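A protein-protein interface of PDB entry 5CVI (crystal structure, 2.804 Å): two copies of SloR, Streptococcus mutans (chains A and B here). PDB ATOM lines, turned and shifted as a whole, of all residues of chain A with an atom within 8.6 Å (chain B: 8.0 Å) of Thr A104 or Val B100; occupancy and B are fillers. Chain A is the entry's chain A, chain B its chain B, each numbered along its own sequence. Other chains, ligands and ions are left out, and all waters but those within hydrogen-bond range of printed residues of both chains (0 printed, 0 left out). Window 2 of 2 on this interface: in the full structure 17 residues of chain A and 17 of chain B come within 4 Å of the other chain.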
ATOM      1  N   ASN A   4     -33.086  17.789 -19.448  1.00  0.00           N
ATOM      2  CA  ASN A   4     -34.184  18.602 -18.931  1.00  0.00           C
ATOM      3  C   ASN A   4     -34.375  19.891 -19.729  1.00  0.00           C
ATOM      4  O   ASN A   4     -33.628  20.165 -20.670  1.00  0.00           O
ATOM      5  CB  ASN A   4     -33.975  18.915 -17.449  1.00  0.00           C
ATOM      6  CG  ASN A   4     -32.709  19.706 -17.192  1.00  0.00           C
ATOM      7  OD1 ASN A   4     -31.741  19.613 -17.949  1.00  0.00           O
ATOM      8  ND2 ASN A   4     -32.708  20.491 -16.116  1.00  0.00           N
ATOM      9  N   GLU A   6     -33.752  22.918 -19.033  1.00  0.00           N
ATOM     10  CA  GLU A   6     -32.633  23.848 -18.920  1.00  0.00           C
ATOM     11  C   GLU A   6     -31.576  23.591 -19.992  1.00  0.00           C
ATOM     12  O   GLU A   6     -30.849  24.501 -20.393  1.00  0.00           O
ATOM     13  CB  GLU A   6     -32.024  23.771 -17.517  1.00  0.00           C
ATOM     14  CG  GLU A   6     -32.999  24.150 -16.411  1.00  0.00           C
ATOM     15  CD  GLU A   6     -32.625  23.564 -15.063  1.00  0.00           C
ATOM     16  OE1 GLU A   6     -33.004  22.404 -14.792  1.00  0.00           O
ATOM     17  OE2 GLU A   6     -31.957  24.264 -14.271  1.00  0.00           O
ATOM     18  N   LEU A  72     -26.058  28.274 -15.666  1.00  0.00           N
ATOM     19  CA  LEU A  72     -25.754  26.924 -16.129  1.00  0.00           C
ATOM     20  C   LEU A  72     -24.339  26.823 -16.682  1.00  0.00           C
ATOM     21  O   LEU A  72     -23.603  25.891 -16.351  1.00  0.00           O
ATOM     22  CB  LEU A  72     -26.763  26.453 -17.177  1.00  0.00           C
ATOM     23  CG  LEU A  72     -27.872  25.528 -16.676  1.00  0.00           C
ATOM     24  CD1 LEU A  72     -27.943  24.270 -17.531  1.00  0.00           C
ATOM     25  CD2 LEU A  72     -27.653  25.169 -15.215  1.00  0.00           C
ATOM     26  N   LYS A  75     -21.791  26.965 -13.743  1.00  0.00           N
ATOM     27  CA  LYS A  75     -21.670  25.653 -13.116  1.00  0.00           C
ATOM     28  C   LYS A  75     -20.835  24.729 -13.988  1.00  0.00           C
ATOM     29  O   LYS A  75     -19.808  24.204 -13.554  1.00  0.00           O
ATOM     30  CB  LYS A  75     -23.043  25.011 -12.916  1.00  0.00           C
ATOM     31  CG  LYS A  75     -23.940  25.660 -11.872  1.00  0.00           C
ATOM     32  CD  LYS A  75     -25.302  24.976 -11.874  1.00  0.00           C
ATOM     33  CE  LYS A  75     -26.221  25.506 -10.787  1.00  0.00           C
ATOM     34  NZ  LYS A  75     -27.453  24.677 -10.659  1.00  0.00           N
ATOM     35  N   ILE A  79     -16.981  23.261 -13.105  1.00  0.00           N
ATOM     36  CA  ILE A  79     -16.843  21.812 -13.007  1.00  0.00           C
ATOM     37  C   ILE A  79     -15.821  21.276 -14.004  1.00  0.00           C
ATOM     38  O   ILE A  79     -15.097  20.328 -13.704  1.00  0.00           O
ATOM     39  CB  ILE A  79     -18.192  21.096 -13.221  1.00  0.00           C
ATOM     40  CG1 ILE A  79     -19.197  21.514 -12.143  1.00  0.00           C
ATOM     41  CG2 ILE A  79     -18.003  19.582 -13.220  1.00  0.00           C
ATOM     42  CD1 ILE A  79     -20.590  20.957 -12.349  1.00  0.00           C
ATOM     43  N   GLU A  97     -20.027  14.070 -17.445  1.00  0.00           N
ATOM     44  CA  GLU A  97     -19.801  14.236 -16.015  1.00  0.00           C
ATOM     45  C   GLU A  97     -20.237  15.624 -15.556  1.00  0.00           C
ATOM     46  O   GLU A  97     -20.979  15.761 -14.583  1.00  0.00           O
ATOM     47  CB  GLU A  97     -18.327  14.015 -15.671  1.00  0.00           C
ATOM     48  CG  GLU A  97     -18.064  13.808 -14.187  1.00  0.00           C
ATOM     49  CD  GLU A  97     -18.486  12.432 -13.716  1.00  0.00           C
ATOM     50  OE1 GLU A  97     -17.775  11.456 -14.034  1.00  0.00           O
ATOM     51  OE2 GLU A  97     -19.529  12.324 -13.036  1.00  0.00           O
ATOM     52  N   ALA A  98     -19.766  16.647 -16.266  1.00  0.00           N
ATOM     53  CA  ALA A  98     -20.093  18.034 -15.941  1.00  0.00           C
ATOM     54  C   ALA A  98     -21.571  18.308 -16.186  1.00  0.00           C
ATOM     55  O   ALA A  98     -22.176  19.167 -15.552  1.00  0.00           O
ATOM     56  CB  ALA A  98     -19.240  18.985 -16.763  1.00  0.00           C
ATOM     57  N   GLU A  99     -22.140  17.566 -17.125  1.00  0.00           N
ATOM     58  CA  GLU A  99     -23.543  17.702 -17.490  1.00  0.00           C
ATOM     59  C   GLU A  99     -24.445  17.247 -16.352  1.00  0.00           C
ATOM     60  O   GLU A  99     -25.430  17.908 -16.026  1.00  0.00           O
ATOM     61  CB  GLU A  99     -23.834  16.891 -18.759  1.00  0.00           C
ATOM     62  CG  GLU A  99     -25.270  16.948 -19.215  1.00  0.00           C
ATOM     63  CD  GLU A  99     -25.781  18.368 -19.321  1.00  0.00           C
ATOM     64  OE1 GLU A  99     -24.992  19.258 -19.707  1.00  0.00           O
ATOM     65  OE2 GLU A  99     -26.970  18.592 -19.014  1.00  0.00           O
ATOM     66  N   VAL A 100     -24.101  16.113 -15.752  1.00  0.00           N
ATOM     67  CA  VAL A 100     -24.863  15.576 -14.630  1.00  0.00           C
ATOM     68  C   VAL A 100     -24.746  16.465 -13.391  1.00  0.00           C
ATOM     69  O   VAL A 100     -25.744  16.769 -12.737  1.00  0.00           O
ATOM     70  CB  VAL A 100     -24.427  14.130 -14.293  1.00  0.00           C
ATOM     71  CG1 VAL A 100     -24.653  13.822 -12.826  1.00  0.00           C
ATOM     72  CG2 VAL A 100     -25.154  13.137 -15.178  1.00  0.00           C
ATOM     73  N   LEU A 101     -23.523  16.887 -13.086  1.00  0.00           N
ATOM     74  CA  LEU A 101     -23.243  17.672 -11.885  1.00  0.00           C
ATOM     75  C   LEU A 101     -23.886  19.059 -11.876  1.00  0.00           C
ATOM     76  O   LEU A 101     -24.273  19.555 -10.816  1.00  0.00           O
ATOM     77  CB  LEU A 101     -21.732  17.798 -11.669  1.00  0.00           C
ATOM     78  CG  LEU A 101     -21.001  16.526 -11.244  1.00  0.00           C
ATOM     79  CD1 LEU A 101     -19.523  16.803 -11.028  1.00  0.00           C
ATOM     80  CD2 LEU A 101     -21.631  15.970  -9.984  1.00  0.00           C
ATOM     81  N   GLU A 102     -23.987  19.687 -13.046  1.00  0.00           N
ATOM     82  CA  GLU A 102     -24.550  21.033 -13.131  1.00  0.00           C
ATOM     83  C   GLU A 102     -26.030  21.040 -12.740  1.00  0.00           C
ATOM     84  O   GLU A 102     -26.587  22.082 -12.395  1.00  0.00           O
ATOM     85  CB  GLU A 102     -24.372  21.625 -14.533  1.00  0.00           C
ATOM     86  CG  GLU A 102     -25.353  21.084 -15.565  1.00  0.00           C
ATOM     87  CD  GLU A 102     -25.236  21.770 -16.917  1.00  0.00           C
ATOM     88  OE1 GLU A 102     -24.251  22.507 -17.140  1.00  0.00           O
ATOM     89  OE2 GLU A 102     -26.135  21.571 -17.760  1.00  0.00           O
ATOM     90  N   HIS A 103     -26.656  19.868 -12.786  1.00  0.00           N
ATOM     91  CA  HIS A 103     -28.065  19.743 -12.429  1.00  0.00           C
ATOM     92  C   HIS A 103     -28.263  19.163 -11.033  1.00  0.00           C
ATOM     93  O   HIS A 103     -29.391  18.956 -10.594  1.00  0.00           O
ATOM     94  CB  HIS A 103     -28.802  18.887 -13.457  1.00  0.00           C
ATOM     95  CG  HIS A 103     -28.872  19.509 -14.815  1.00  0.00           C
ATOM     96  ND1 HIS A 103     -29.512  20.705 -15.053  1.00  0.00           N
ATOM     97  CD2 HIS A 103     -28.383  19.097 -16.007  1.00  0.00           C
ATOM     98  CE1 HIS A 103     -29.413  21.006 -16.335  1.00  0.00           C
ATOM     99  NE2 HIS A 103     -28.735  20.047 -16.937  1.00  0.00           N
ATOM    100  N   THR A 104     -27.161  18.899 -10.341  1.00  0.00           N
ATOM    101  CA  THR A 104     -27.217  18.317  -9.007  1.00  0.00           C
ATOM    102  C   THR A 104     -26.083  18.842  -8.147  1.00  0.00           C
ATOM    103  O   THR A 104     -25.203  18.088  -7.743  1.00  0.00           O
ATOM    104  CB  THR A 104     -27.102  16.786  -9.063  1.00  0.00           C
ATOM    105  OG1 THR A 104     -25.857  16.424  -9.672  1.00  0.00           O
ATOM    106  CG2 THR A 104     -28.247  16.189  -9.875  1.00  0.00           C
ATOM    107  N   VAL A 105     -26.104  20.140  -7.875  1.00  0.00           N
ATOM    108  CA  VAL A 105     -25.059  20.778  -7.086  1.00  0.00           C
ATOM    109  C   VAL A 105     -25.552  22.114  -6.559  1.00  0.00           C
ATOM    110  O   VAL A 105     -26.099  22.923  -7.309  1.00  0.00           O
ATOM    111  CB  VAL A 105     -23.777  21.003  -7.909  1.00  0.00           C
ATOM    112  CG1 VAL A 105     -23.105  22.294  -7.493  1.00  0.00           C
ATOM    113  CG2 VAL A 105     -22.831  19.825  -7.754  1.00  0.00           C
ATOM    114  N   SER A 106     -25.360  22.345  -5.267  1.00  0.00           N
ATOM    115  CA  SER A 106     -25.862  23.557  -4.637  1.00  0.00           C
ATOM    116  C   SER A 106     -25.051  24.770  -5.062  1.00  0.00           C
ATOM    117  O   SER A 106     -23.908  24.642  -5.510  1.00  0.00           O
ATOM    118  CB  SER A 106     -25.842  23.426  -3.113  1.00  0.00           C
ATOM    119  OG  SER A 106     -24.518  23.337  -2.622  1.00  0.00           O
ATOM    120  N   ASP A 107     -25.658  25.945  -4.925  1.00  0.00           N
ATOM    121  CA  ASP A 107     -24.968  27.188  -5.226  1.00  0.00           C
ATOM    122  C   ASP A 107     -23.780  27.360  -4.288  1.00  0.00           C
ATOM    123  O   ASP A 107     -22.784  27.988  -4.642  1.00  0.00           O
ATOM    124  CB  ASP A 107     -25.921  28.382  -5.118  1.00  0.00           C
ATOM    125  CG  ASP A 107     -26.879  28.479  -6.297  1.00  0.00           C
ATOM    126  OD1 ASP A 107     -26.486  28.102  -7.423  1.00  0.00           O
ATOM    127  OD2 ASP A 107     -28.026  28.938  -6.098  1.00  0.00           O
ATOM    128  N   PHE A 109     -21.887  24.867  -3.198  1.00  0.00           N
ATOM    129  CA  PHE A 109     -20.849  24.044  -3.808  1.00  0.00           C
ATOM    130  C   PHE A 109     -20.162  24.807  -4.928  1.00  0.00           C
ATOM    131  O   PHE A 109     -18.930  24.859  -4.996  1.00  0.00           O
ATOM    132  CB  PHE A 109     -21.437  22.750  -4.369  1.00  0.00           C
ATOM    133  CG  PHE A 109     -20.414  21.837  -4.993  1.00  0.00           C
ATOM    134  CD1 PHE A 109     -20.071  21.961  -6.332  1.00  0.00           C
ATOM    135  CD2 PHE A 109     -19.800  20.851  -4.239  1.00  0.00           C
ATOM    136  CE1 PHE A 109     -19.131  21.119  -6.903  1.00  0.00           C
ATOM    137  CE2 PHE A 109     -18.861  20.011  -4.804  1.00  0.00           C
ATOM    138  CZ  PHE A 109     -18.528  20.143  -6.136  1.00  0.00           C
ATOM    139  N   VAL A 110     -20.968  25.392  -5.812  1.00  0.00           N
ATOM    140  CA  VAL A 110     -20.438  26.121  -6.957  1.00  0.00           C
ATOM    141  C   VAL A 110     -19.608  27.319  -6.508  1.00  0.00           C
ATOM    142  O   VAL A 110     -18.565  27.616  -7.088  1.00  0.00           O
ATOM    143  CB  VAL A 110     -21.561  26.592  -7.894  1.00  0.00           C
ATOM    144  CG1 VAL A 110     -20.987  27.375  -9.055  1.00  0.00           C
ATOM    145  CG2 VAL A 110     -22.360  25.397  -8.400  1.00  0.00           C
ATOM    146  N   MET B   1     -33.737  18.874  -1.282  1.00  0.00           N
ATOM    147  CA  MET B   1     -32.992  17.623  -1.202  1.00  0.00           C
ATOM    148  C   MET B   1     -33.889  16.505  -0.677  1.00  0.00           C
ATOM    149  O   MET B   1     -34.354  16.556   0.463  1.00  0.00           O
ATOM    150  CB  MET B   1     -31.761  17.797  -0.305  1.00  0.00           C
ATOM    151  CG  MET B   1     -30.752  16.656  -0.370  1.00  0.00           C
ATOM    152  SD  MET B   1     -31.225  15.114   0.728  1.00  0.00           S
ATOM    153  CE  MET B   1     -31.176  15.965   2.482  1.00  0.00           C
ATOM    154  N   THR B   2     -34.137  15.499  -1.514  1.00  0.00           N
ATOM    155  CA  THR B   2     -34.969  14.362  -1.124  1.00  0.00           C
ATOM    156  C   THR B   2     -34.192  13.048  -1.174  1.00  0.00           C
ATOM    157  O   THR B   2     -33.718  12.642  -2.237  1.00  0.00           O
ATOM    158  CB  THR B   2     -36.215  14.230  -2.023  1.00  0.00           C
ATOM    159  OG1 THR B   2     -36.980  15.441  -1.971  1.00  0.00           O
ATOM    160  CG2 THR B   2     -37.083  13.064  -1.566  1.00  0.00           C
ATOM    161  N   PRO B   3     -34.058  12.377  -0.020  1.00  0.00           N
ATOM    162  CA  PRO B   3     -33.373  11.080   0.038  1.00  0.00           C
ATOM    163  C   PRO B   3     -34.160  10.031  -0.736  1.00  0.00           C
ATOM    164  O   PRO B   3     -35.368   9.916  -0.529  1.00  0.00           O
ATOM    165  CB  PRO B   3     -33.389  10.737   1.534  1.00  0.00           C
ATOM    166  CG  PRO B   3     -33.679  12.023   2.238  1.00  0.00           C
ATOM    167  CD  PRO B   3     -34.541  12.805   1.303  1.00  0.00           C
ATOM    168  N   ASP B   7     -31.212   4.983   0.524  1.00  0.00           N
ATOM    169  CA  ASP B   7     -30.690   5.396   1.824  1.00  0.00           C
ATOM    170  C   ASP B   7     -31.210   4.530   2.967  1.00  0.00           C
ATOM    171  O   ASP B   7     -30.618   4.481   4.044  1.00  0.00           O
ATOM    172  CB  ASP B   7     -31.011   6.866   2.086  1.00  0.00           C
ATOM    173  CG  ASP B   7     -30.305   7.790   1.122  1.00  0.00           C
ATOM    174  OD1 ASP B   7     -29.228   7.405   0.624  1.00  0.00           O
ATOM    175  OD2 ASP B   7     -30.826   8.893   0.859  1.00  0.00           O
ATOM    176  N   HIS B  76     -20.224   8.207  -0.170  1.00  0.00           N
ATOM    177  CA  HIS B  76     -20.660   9.205   0.799  1.00  0.00           C
ATOM    178  C   HIS B  76     -19.495   9.750   1.615  1.00  0.00           C
ATOM    179  O   HIS B  76     -19.388  10.953   1.837  1.00  0.00           O
ATOM    180  CB  HIS B  76     -21.714   8.621   1.744  1.00  0.00           C
ATOM    181  CG  HIS B  76     -22.358   9.642   2.631  1.00  0.00           C
ATOM    182  ND1 HIS B  76     -23.429  10.409   2.225  1.00  0.00           N
ATOM    183  CD2 HIS B  76     -22.071  10.034   3.895  1.00  0.00           C
ATOM    184  CE1 HIS B  76     -23.781  11.223   3.205  1.00  0.00           C
ATOM    185  NE2 HIS B  76     -22.973  11.016   4.229  1.00  0.00           N
ATOM    186  N   ILE B  79     -16.793  11.611  -0.500  1.00  0.00           N
ATOM    187  CA  ILE B  79     -17.280  12.936  -0.875  1.00  0.00           C
ATOM    188  C   ILE B  79     -17.204  13.941   0.266  1.00  0.00           C
ATOM    189  O   ILE B  79     -16.901  15.116   0.042  1.00  0.00           O
ATOM    190  CB  ILE B  79     -18.733  12.893  -1.392  1.00  0.00           C
ATOM    191  CG1 ILE B  79     -18.798  12.215  -2.762  1.00  0.00           C
ATOM    192  CG2 ILE B  79     -19.310  14.298  -1.485  1.00  0.00           C
ATOM    193  CD1 ILE B  79     -20.208  12.023  -3.274  1.00  0.00           C
ATOM    194  N   ILE B  94     -22.024  19.089   5.364  1.00  0.00           N
ATOM    195  CA  ILE B  94     -21.544  18.032   4.477  1.00  0.00           C
ATOM    196  C   ILE B  94     -22.604  17.012   4.070  1.00  0.00           C
ATOM    197  O   ILE B  94     -22.629  16.576   2.918  1.00  0.00           O
ATOM    198  CB  ILE B  94     -20.333  17.288   5.083  1.00  0.00           C
ATOM    199  CG1 ILE B  94     -20.696  16.721   6.455  1.00  0.00           C
ATOM    200  CG2 ILE B  94     -19.134  18.219   5.181  1.00  0.00           C
ATOM    201  CD1 ILE B  94     -19.546  16.057   7.169  1.00  0.00           C
ATOM    202  N   HIS B  95     -23.472  16.627   5.001  1.00  0.00           N
ATOM    203  CA  HIS B  95     -24.385  15.515   4.741  1.00  0.00           C
ATOM    204  C   HIS B  95     -25.317  15.721   3.549  1.00  0.00           C
ATOM    205  O   HIS B  95     -25.443  14.843   2.697  1.00  0.00           O
ATOM    206  CB  HIS B  95     -25.217  15.156   5.970  1.00  0.00           C
ATOM    207  CG  HIS B  95     -26.164  14.025   5.725  1.00  0.00           C
ATOM    208  ND1 HIS B  95     -25.738  12.722   5.571  1.00  0.00           N
ATOM    209  CD2 HIS B  95     -27.507  14.002   5.563  1.00  0.00           C
ATOM    210  CE1 HIS B  95     -26.779  11.943   5.348  1.00  0.00           C
ATOM    211  NE2 HIS B  95     -27.866  12.695   5.338  1.00  0.00           N
ATOM    212  N   GLU B  96     -25.974  16.874   3.498  1.00  0.00           N
ATOM    213  CA  GLU B  96     -26.927  17.161   2.429  1.00  0.00           C
ATOM    214  C   GLU B  96     -26.267  17.235   1.047  1.00  0.00           C
ATOM    215  O   GLU B  96     -26.857  16.829   0.048  1.00  0.00           O
ATOM    216  CB  GLU B  96     -27.717  18.441   2.727  1.00  0.00           C
ATOM    217  CG  GLU B  96     -27.031  19.395   3.699  1.00  0.00           C
ATOM    218  CD  GLU B  96     -27.185  18.973   5.152  1.00  0.00           C
ATOM    219  OE1 GLU B  96     -28.263  18.454   5.516  1.00  0.00           O
ATOM    220  OE2 GLU B  96     -26.225  19.160   5.930  1.00  0.00           O
ATOM    221  N   GLU B  97     -25.039  17.740   0.996  1.00  0.00           N
ATOM    222  CA  GLU B  97     -24.317  17.854  -0.267  1.00  0.00           C
ATOM    223  C   GLU B  97     -23.783  16.499  -0.731  1.00  0.00           C
ATOM    224  O   GLU B  97     -23.902  16.142  -1.907  1.00  0.00           O
ATOM    225  CB  GLU B  97     -23.166  18.855  -0.143  1.00  0.00           C
ATOM    226  CG  GLU B  97     -22.576  19.283  -1.471  1.00  0.00           C
ATOM    227  CD  GLU B  97     -23.478  20.249  -2.219  1.00  0.00           C
ATOM    228  OE1 GLU B  97     -23.800  21.317  -1.654  1.00  0.00           O
ATOM    229  OE2 GLU B  97     -23.866  19.943  -3.369  1.00  0.00           O
ATOM    230  N   ALA B  98     -23.193  15.755   0.201  1.00  0.00           N
ATOM    231  CA  ALA B  98     -22.619  14.447  -0.101  1.00  0.00           C
ATOM    232  C   ALA B  98     -23.714  13.443  -0.437  1.00  0.00           C
ATOM    233  O   ALA B  98     -23.459  12.382  -1.003  1.00  0.00           O
ATOM    234  CB  ALA B  98     -21.797  13.951   1.074  1.00  0.00           C
ATOM    235  N   GLU B  99     -24.938  13.795  -0.074  1.00  0.00           N
ATOM    236  CA  GLU B  99     -26.092  12.927  -0.245  1.00  0.00           C
ATOM    237  C   GLU B  99     -26.560  12.967  -1.693  1.00  0.00           C
ATOM    238  O   GLU B  99     -26.773  11.929  -2.320  1.00  0.00           O
ATOM    239  CB  GLU B  99     -27.208  13.384   0.700  1.00  0.00           C
ATOM    240  CG  GLU B  99     -28.342  12.405   0.852  1.00  0.00           C
ATOM    241  CD  GLU B  99     -27.869  11.032   1.267  1.00  0.00           C
ATOM    242  OE1 GLU B  99     -27.167  10.915   2.294  1.00  0.00           O
ATOM    243  OE2 GLU B  99     -28.195  10.063   0.555  1.00  0.00           O
ATOM    244  N   VAL B 100     -26.711  14.180  -2.214  1.00  0.00           N
ATOM    245  CA  VAL B 100     -27.086  14.388  -3.606  1.00  0.00           C
ATOM    246  C   VAL B 100     -26.021  13.841  -4.554  1.00  0.00           C
ATOM    247  O   VAL B 100     -26.341  13.253  -5.588  1.00  0.00           O
ATOM    248  CB  VAL B 100     -27.314  15.887  -3.900  1.00  0.00           C
ATOM    249  CG1 VAL B 100     -27.399  16.136  -5.396  1.00  0.00           C
ATOM    250  CG2 VAL B 100     -28.568  16.384  -3.195  1.00  0.00           C
ATOM    251  N   LEU B 101     -24.755  14.022  -4.188  1.00  0.00           N
ATOM    252  CA  LEU B 101     -23.642  13.638  -5.054  1.00  0.00           C
ATOM    253  C   LEU B 101     -23.405  12.130  -5.121  1.00  0.00           C
ATOM    254  O   LEU B 101     -22.904  11.624  -6.128  1.00  0.00           O
ATOM    255  CB  LEU B 101     -22.359  14.372  -4.649  1.00  0.00           C
ATOM    256  CG  LEU B 101     -22.429  15.894  -4.798  1.00  0.00           C
ATOM    257  CD1 LEU B 101     -21.112  16.563  -4.419  1.00  0.00           C
ATOM    258  CD2 LEU B 101     -22.823  16.257  -6.217  1.00  0.00           C
ATOM    259  N   GLU B 102     -23.766  11.412  -4.062  1.00  0.00           N
ATOM    260  CA  GLU B 102     -23.539   9.969  -4.028  1.00  0.00           C
ATOM    261  C   GLU B 102     -24.458   9.213  -4.992  1.00  0.00           C
ATOM    262  O   GLU B 102     -24.260   8.028  -5.245  1.00  0.00           O
ATOM    263  CB  GLU B 102     -23.673   9.415  -2.606  1.00  0.00           C
ATOM    264  CG  GLU B 102     -25.094   9.373  -2.065  1.00  0.00           C
ATOM    265  CD  GLU B 102     -25.185   8.686  -0.708  1.00  0.00           C
ATOM    266  OE1 GLU B 102     -24.240   8.819   0.101  1.00  0.00           O
ATOM    267  OE2 GLU B 102     -26.200   8.006  -0.456  1.00  0.00           O
ATOM    268  N   HIS B 103     -25.452   9.910  -5.534  1.00  0.00           N
ATOM    269  CA  HIS B 103     -26.399   9.310  -6.471  1.00  0.00           C
ATOM    270  C   HIS B 103     -26.222   9.853  -7.885  1.00  0.00           C
ATOM    271  O   HIS B 103     -26.872   9.392  -8.825  1.00  0.00           O
ATOM    272  CB  HIS B 103     -27.834   9.549  -6.008  1.00  0.00           C
ATOM    273  CG  HIS B 103     -28.150   8.926  -4.687  1.00  0.00           C
ATOM    274  ND1 HIS B 103     -28.183   7.563  -4.498  1.00  0.00           N
ATOM    275  CD2 HIS B 103     -28.445   9.481  -3.487  1.00  0.00           C
ATOM    276  CE1 HIS B 103     -28.485   7.302  -3.238  1.00  0.00           C
ATOM    277  NE2 HIS B 103     -28.654   8.449  -2.605  1.00  0.00           N
ATOM    278  N   THR B 104     -25.341  10.839  -8.026  1.00  0.00           N
ATOM    279  CA  THR B 104     -25.116  11.491  -9.309  1.00  0.00           C
ATOM    280  C   THR B 104     -23.631  11.701  -9.556  1.00  0.00           C
ATOM    281  O   THR B 104     -23.186  12.824  -9.779  1.00  0.00           O
ATOM    282  CB  THR B 104     -25.820  12.859  -9.372  1.00  0.00           C
ATOM    283  OG1 THR B 104     -25.212  13.751  -8.431  1.00  0.00           O
ATOM    284  CG2 THR B 104     -27.303  12.718  -9.041  1.00  0.00           C
ATOM    285  N   VAL B 105     -22.867  10.617  -9.507  1.00  0.00           N
ATOM    286  CA  VAL B 105     -21.425  10.685  -9.703  1.00  0.00           C
ATOM    287  C   VAL B 105     -20.904   9.366 -10.267  1.00  0.00           C
ATOM    288  O   VAL B 105     -21.160   8.297  -9.705  1.00  0.00           O
ATOM    289  CB  VAL B 105     -20.693  11.024  -8.388  1.00  0.00           C
ATOM    290  CG1 VAL B 105     -19.334  10.365  -8.345  1.00  0.00           C
ATOM    291  CG2 VAL B 105     -20.575  12.530  -8.223  1.00  0.00           C
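OE2 of Glu B97 sits at hydrogen-bond distance from N of Ser A106 (3.4 Å). OG1 of Thr A104 is in hydrogen-bond range of OG1 of Thr B104, 3.0 Å away.
The backbone carbonyl oxygen (O) of Val A100 lies within hydrogen-bond range of the side-chain hydroxyl (OG1) of Thr A104 (3.1 Å). OG of Ser A106 lies within hydrogen-bond range of N of Phe A109 (3.1 Å). O of Val B100 sits at hydrogen-bond distance from OG1 of Thr B104 (3.1 Å).
Thr B104 touches Val A100. CD2 of Leu A101 touches CD2 of Leu B101, 3.96 Å away. Thr B104 touches Leu A101. Val B100 touches Thr A104 (CG1 to CB, 3.7 Å). Thr A104 touches Leu B101. Val A105 touches Glu B97. Leu B101 touches Val A105 (CD2 to CG2, 3.9 Å). CB of Phe A109 touches OE2 of Glu B97 (3.8 Å).
Glu A6 touches none of the printed residues of chain B. Of chain B, only Val B100 (3.7 Å), Leu B101 (3.4 Å) and Thr B104 (3.0 Å) come within 4 Å of Thr A104. Of the printed residues of chain B, Ser A106 touches Glu B97. Glu B99 touches none of the printed residues of chain A. Val B100 touches one residue of chain A. Printed residues of chain A within 4 Å of Leu B101: Leu A101, Thr A104 and Val A105. The nearest residue of chain B that does not touch Thr A104 is Glu B97 (4.9 Å). The nearest residue of chain A that does not touch Val B100 is Val A105 (4.9 Å).
Hydrophobic or aromatic side chains of chain B within 4 Å of the printed part of chain A: Val B100 and Leu B101. Hydrophobic or aromatic side chains of chain A within 4 Å of the printed part of chain B: Val A100, Leu A101, Val A105 and Phe A109. Among the printed residues, 10 pairs touch across the chains. Among the printed residues, no Asp or Glu carboxylate lies within 4 Å of a Lys or Arg side-chain nitrogen of the other chain.
Val A100 touches Thr B104, and with the chains exchanged Thr A104 touches Val B100. Leu A101 touches Thr B104, and with the chains exchanged Thr A104 touches Leu B101. Thr A104 touches its own counterpart, Thr B104. Val A105 touches Leu B101, but with the chains exchanged Leu A101 does not touch Val B105 (4.01 Å).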
